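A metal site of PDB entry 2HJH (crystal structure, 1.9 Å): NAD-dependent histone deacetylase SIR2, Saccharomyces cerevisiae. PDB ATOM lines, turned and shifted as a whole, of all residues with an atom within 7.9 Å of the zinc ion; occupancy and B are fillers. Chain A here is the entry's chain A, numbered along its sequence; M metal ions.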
ATOM      1  N   THR A 163      19.886  26.803 -28.894  1.00  0.00           N
ATOM      2  CA  THR A 163      20.701  25.883 -28.156  1.00  0.00           C
ATOM      3  C   THR A 163      19.890  24.892 -27.281  1.00  0.00           C
ATOM      4  O   THR A 163      18.984  25.304 -26.544  1.00  0.00           O
ATOM      5  CB  THR A 163      21.668  26.675 -27.251  1.00  0.00           C
ATOM      6  OG1 THR A 163      22.545  27.458 -28.074  1.00  0.00           O
ATOM      7  CG2 THR A 163      22.615  25.724 -26.532  1.00  0.00           C
ATOM      8  N   CYS A 164      20.225  23.598 -27.280  1.00  0.00           N
ATOM      9  CA  CYS A 164      19.582  22.680 -26.351  1.00  0.00           C
ATOM     10  C   CYS A 164      20.001  23.010 -24.915  1.00  0.00           C
ATOM     11  O   CYS A 164      21.213  23.067 -24.644  1.00  0.00           O
ATOM     12  CB  CYS A 164      19.918  21.232 -26.676  1.00  0.00           C
ATOM     13  SG  CYS A 164      19.210  20.148 -25.446  1.00  0.00           S
ATOM     14  N   VAL A 165      19.064  23.217 -24.014  1.00  0.00           N
ATOM     15  CA  VAL A 165      19.473  23.533 -22.628  1.00  0.00           C
ATOM     16  C   VAL A 165      20.083  22.401 -21.823  1.00  0.00           C
ATOM     17  O   VAL A 165      20.674  22.632 -20.728  1.00  0.00           O
ATOM     18  CB  VAL A 165      18.365  24.180 -21.784  1.00  0.00           C
ATOM     19  CG1 VAL A 165      17.825  25.500 -22.486  1.00  0.00           C
ATOM     20  CG2 VAL A 165      17.275  23.175 -21.490  1.00  0.00           C
ATOM     21  N   THR A 166      19.968  21.186 -22.322  1.00  0.00           N
ATOM     22  CA  THR A 166      20.533  20.012 -21.670  1.00  0.00           C
ATOM     23  C   THR A 166      21.923  19.605 -22.203  1.00  0.00           C
ATOM     24  O   THR A 166      22.839  19.441 -21.445  1.00  0.00           O
ATOM     25  CB  THR A 166      19.513  18.852 -21.832  1.00  0.00           C
ATOM     26  OG1 THR A 166      18.245  19.198 -21.247  1.00  0.00           O
ATOM     27  CG2 THR A 166      19.907  17.664 -21.116  1.00  0.00           C
ATOM     28  N   CYS A 167      22.042  19.382 -23.518  1.00  0.00           N
ATOM     29  CA  CYS A 167      23.247  18.893 -24.144  1.00  0.00           C
ATOM     30  C   CYS A 167      24.041  19.993 -24.845  1.00  0.00           C
ATOM     31  O   CYS A 167      25.144  19.730 -25.314  1.00  0.00           O
ATOM     32  CB  CYS A 167      23.016  17.738 -25.094  1.00  0.00           C
ATOM     33  SG  CYS A 167      22.310  18.230 -26.701  1.00  0.00           S
ATOM     34  N   HIS A 168      23.473  21.168 -24.982  1.00  0.00           N
ATOM     35  CA  HIS A 168      24.180  22.306 -25.590  1.00  0.00           C
ATOM     36  C   HIS A 168      24.400  22.224 -27.062  1.00  0.00           C
ATOM     37  O   HIS A 168      25.055  23.064 -27.656  1.00  0.00           O
ATOM     38  CB  HIS A 168      25.493  22.659 -24.826  1.00  0.00           C
ATOM     39  CG  HIS A 168      25.377  22.547 -23.333  1.00  0.00           C
ATOM     40  ND1 HIS A 168      24.590  23.370 -22.562  1.00  0.00           N
ATOM     41  CD2 HIS A 168      25.887  21.622 -22.475  1.00  0.00           C
ATOM     42  CE1 HIS A 168      24.624  22.979 -21.306  1.00  0.00           C
ATOM     43  NE2 HIS A 168      25.397  21.910 -21.216  1.00  0.00           N
ATOM     44  N   TRP A 169      23.802  21.268 -27.713  1.00  0.00           N
ATOM     45  CA  TRP A 169      23.765  21.295 -29.184  1.00  0.00           C
ATOM     46  C   TRP A 169      23.239  22.684 -29.677  1.00  0.00           C
ATOM     47  O   TRP A 169      22.225  23.177 -29.161  1.00  0.00           O
ATOM     48  CB  TRP A 169      22.871  20.177 -29.693  1.00  0.00           C
ATOM     49  CG  TRP A 169      22.886  20.056 -31.168  1.00  0.00           C
ATOM     50  CD1 TRP A 169      23.982  19.803 -31.996  1.00  0.00           C
ATOM     51  CD2 TRP A 169      21.758  20.150 -32.030  1.00  0.00           C
ATOM     52  NE1 TRP A 169      23.578  19.723 -33.304  1.00  0.00           N
ATOM     53  CE2 TRP A 169      22.219  19.922 -33.361  1.00  0.00           C
ATOM     54  CE3 TRP A 169      20.408  20.312 -31.819  1.00  0.00           C
ATOM     55  CZ2 TRP A 169      21.364  19.903 -34.468  1.00  0.00           C
ATOM     56  CZ3 TRP A 169      19.567  20.346 -32.901  1.00  0.00           C
ATOM     57  CH2 TRP A 169      20.054  20.099 -34.226  1.00  0.00           C
ATOM     58  N   ASN A 170      23.900  23.261 -30.671  1.00  0.00           N
ATOM     59  CA  ASN A 170      23.632  24.624 -31.240  1.00  0.00           C
ATOM     60  C   ASN A 170      23.203  24.441 -32.720  1.00  0.00           C
ATOM     61  O   ASN A 170      23.771  23.629 -33.457  1.00  0.00           O
ATOM     62  CB  ASN A 170      24.891  25.497 -31.149  1.00  0.00           C
ATOM     63  CG  ASN A 170      24.638  27.024 -31.451  1.00  0.00           C
ATOM     64  OD1 ASN A 170      24.980  27.479 -32.555  1.00  0.00           O
ATOM     65  ND2 ASN A 170      24.127  27.796 -30.471  1.00  0.00           N
ATOM     66  N   LEU A 187      12.164  20.542 -29.854  1.00  0.00           N
ATOM     67  CA  LEU A 187      12.856  19.550 -29.066  1.00  0.00           C
ATOM     68  C   LEU A 187      14.172  19.245 -29.690  1.00  0.00           C
ATOM     69  O   LEU A 187      14.320  19.177 -30.917  1.00  0.00           O
ATOM     70  CB  LEU A 187      12.020  18.282 -28.943  1.00  0.00           C
ATOM     71  CG  LEU A 187      10.744  18.481 -28.158  1.00  0.00           C
ATOM     72  CD1 LEU A 187       9.947  17.229 -28.014  1.00  0.00           C
ATOM     73  CD2 LEU A 187      11.079  19.054 -26.827  1.00  0.00           C
ATOM     74  N   CYS A 188      15.123  18.955 -28.833  1.00  0.00           N
ATOM     75  CA  CYS A 188      16.414  18.489 -29.266  1.00  0.00           C
ATOM     76  C   CYS A 188      16.410  17.097 -29.792  1.00  0.00           C
ATOM     77  O   CYS A 188      15.972  16.151 -29.117  1.00  0.00           O
ATOM     78  CB  CYS A 188      17.401  18.635 -28.108  1.00  0.00           C
ATOM     79  SG  CYS A 188      19.045  18.031 -28.555  1.00  0.00           S
ATOM     80  N   PRO A 189      16.942  16.905 -31.006  1.00  0.00           N
ATOM     81  CA  PRO A 189      16.957  15.548 -31.575  1.00  0.00           C
ATOM     82  C   PRO A 189      17.883  14.565 -30.894  1.00  0.00           C
ATOM     83  O   PRO A 189      17.625  13.374 -30.939  1.00  0.00           O
ATOM     84  CB  PRO A 189      17.395  15.772 -33.056  1.00  0.00           C
ATOM     85  CG  PRO A 189      18.013  17.053 -33.109  1.00  0.00           C
ATOM     86  CD  PRO A 189      17.523  17.889 -31.931  1.00  0.00           C
ATOM     87  N   TYR A 190      18.924  15.039 -30.221  1.00  0.00           N
ATOM     88  CA  TYR A 190      19.825  14.169 -29.488  1.00  0.00           C
ATOM     89  C   TYR A 190      19.298  13.782 -28.105  1.00  0.00           C
ATOM     90  O   TYR A 190      19.532  12.668 -27.643  1.00  0.00           O
ATOM     91  CB  TYR A 190      21.222  14.833 -29.342  1.00  0.00           C
ATOM     92  CG  TYR A 190      21.882  15.035 -30.648  1.00  0.00           C
ATOM     93  CD1 TYR A 190      21.911  16.260 -31.218  1.00  0.00           C
ATOM     94  CD2 TYR A 190      22.430  13.962 -31.362  1.00  0.00           C
ATOM     95  CE1 TYR A 190      22.485  16.446 -32.439  1.00  0.00           C
ATOM     96  CE2 TYR A 190      23.007  14.163 -32.607  1.00  0.00           C
ATOM     97  CZ  TYR A 190      22.996  15.412 -33.131  1.00  0.00           C
ATOM     98  OH  TYR A 190      23.593  15.707 -34.343  1.00  0.00           O
ATOM     99  N   CYS A 191      18.614  14.696 -27.429  1.00  0.00           N
ATOM    100  CA  CYS A 191      18.052  14.430 -26.099  1.00  0.00           C
ATOM    101  C   CYS A 191      16.642  13.714 -26.236  1.00  0.00           C
ATOM    102  O   CYS A 191      16.033  13.318 -25.260  1.00  0.00           O
ATOM    103  CB  CYS A 191      17.909  15.749 -25.344  1.00  0.00           C
ATOM    104  SG  CYS A 191      19.504  16.446 -24.818  1.00  0.00           S
ATOM    105  N   TYR A 192      16.161  13.576 -27.451  1.00  0.00           N
ATOM    106  CA  TYR A 192      14.770  13.234 -27.641  1.00  0.00           C
ATOM    107  C   TYR A 192      14.387  11.863 -27.057  1.00  0.00           C
ATOM    108  O   TYR A 192      13.339  11.717 -26.477  1.00  0.00           O
ATOM    109  CB  TYR A 192      14.500  13.225 -29.114  1.00  0.00           C
ATOM    110  CG  TYR A 192      13.052  12.971 -29.510  1.00  0.00           C
ATOM    111  CD1 TYR A 192      12.100  13.942 -29.322  1.00  0.00           C
ATOM    112  CD2 TYR A 192      12.679  11.774 -30.130  1.00  0.00           C
ATOM    113  CE1 TYR A 192      10.790  13.760 -29.733  1.00  0.00           C
ATOM    114  CE2 TYR A 192      11.354  11.532 -30.536  1.00  0.00           C
ATOM    115  CZ  TYR A 192      10.415  12.547 -30.345  1.00  0.00           C
ATOM    116  OH  TYR A 192       9.106  12.375 -30.734  1.00  0.00           O
ATOM    117  N   TYR A 227      13.788  19.862 -19.982  1.00  0.00           N
ATOM    118  CA  TYR A 227      14.728  18.784 -20.377  1.00  0.00           C
ATOM    119  C   TYR A 227      14.742  18.553 -21.885  1.00  0.00           C
ATOM    120  O   TYR A 227      13.660  18.303 -22.508  1.00  0.00           O
ATOM    121  CB  TYR A 227      14.409  17.492 -19.650  1.00  0.00           C
ATOM    122  CG  TYR A 227      15.449  16.453 -19.941  1.00  0.00           C
ATOM    123  CD1 TYR A 227      16.544  16.283 -19.102  1.00  0.00           C
ATOM    124  CD2 TYR A 227      15.375  15.653 -21.063  1.00  0.00           C
ATOM    125  CE1 TYR A 227      17.502  15.379 -19.399  1.00  0.00           C
ATOM    126  CE2 TYR A 227      16.403  14.740 -21.362  1.00  0.00           C
ATOM    127  CZ  TYR A 227      17.430  14.602 -20.540  1.00  0.00           C
ATOM    128  OH  TYR A 227      18.440  13.652 -20.795  1.00  0.00           O
ATOM    129  N   GLY A 228      15.860  18.709 -22.555  1.00  0.00           N
ATOM    130  CA  GLY A 228      15.910  18.472 -24.023  1.00  0.00           C
ATOM    131  C   GLY A 228      15.081  19.424 -24.925  1.00  0.00           C
ATOM    132  O   GLY A 228      14.726  19.097 -26.075  1.00  0.00           O
ATOM    133  N   VAL A 229      14.837  20.621 -24.408  1.00  0.00           N
ATOM    134  CA  VAL A 229      14.208  21.704 -25.128  1.00  0.00           C
ATOM    135  C   VAL A 229      15.229  22.660 -25.671  1.00  0.00           C
ATOM    136  O   VAL A 229      16.104  23.119 -24.992  1.00  0.00           O
ATOM    137  CB  VAL A 229      13.156  22.391 -24.248  1.00  0.00           C
ATOM    138  CG1 VAL A 229      12.407  23.544 -25.014  1.00  0.00           C
ATOM    139  CG2 VAL A 229      12.126  21.326 -23.813  1.00  0.00           C
ATOM    140  N   LEU A 230      15.067  23.004 -26.955  1.00  0.00           N
ATOM    141  CA  LEU A 230      15.825  24.087 -27.545  1.00  0.00           C
ATOM    142  C   LEU A 230      15.318  25.461 -27.117  1.00  0.00           C
ATOM    143  O   LEU A 230      14.089  25.705 -27.048  1.00  0.00           O
ATOM    144  CB  LEU A 230      15.849  23.930 -29.040  1.00  0.00           C
ATOM    145  CG  LEU A 230      16.204  22.538 -29.479  1.00  0.00           C
ATOM    146  CD1 LEU A 230      15.868  22.404 -30.907  1.00  0.00           C
ATOM    147  CD2 LEU A 230      17.655  22.320 -29.337  1.00  0.00           C
HETATM  148 ZN    ZN M   1      20.018  18.119 -26.437  1.00  0.00          ZN
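The side-chain sulfur of Cys 167 lies close to the backbone NH of Trp 169 (3.5 Å).
The backbone NH of Thr 166 sits close to the side-chain sulfur of Cys 164 (3.4 Å).
The backbone NH of Cys 188 sits at hydrogen-bond distance from the backbone carbonyl oxygen of Gly 228.
The side-chain sulfur (SG) of Cys 188 sits close to the backbone NH (N) of Tyr 190 (3.4 Å).
N of Cys 164 sits at hydrogen-bond distance from O of Trp 169 (2.8 Å).
Four residues have an atom within 4 Å of the zinc ion: Cys 164, Cys 167, Cys 188 and Cys 191.
The nearest printed residue that does not touch the zinc ion is Tyr 190 (4.5 Å).
The side-chain sulfur (SG) of Cys 167 is bound to the zinc ion (2.3 Å).
SG of Cys 188 binds the zinc ion, 2.3 Å away.
The side-chain sulfur (SG) of Cys 191 binds the zinc ion.
The side-chain sulfur (SG) of Cys 164 is bound to the zinc ion.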
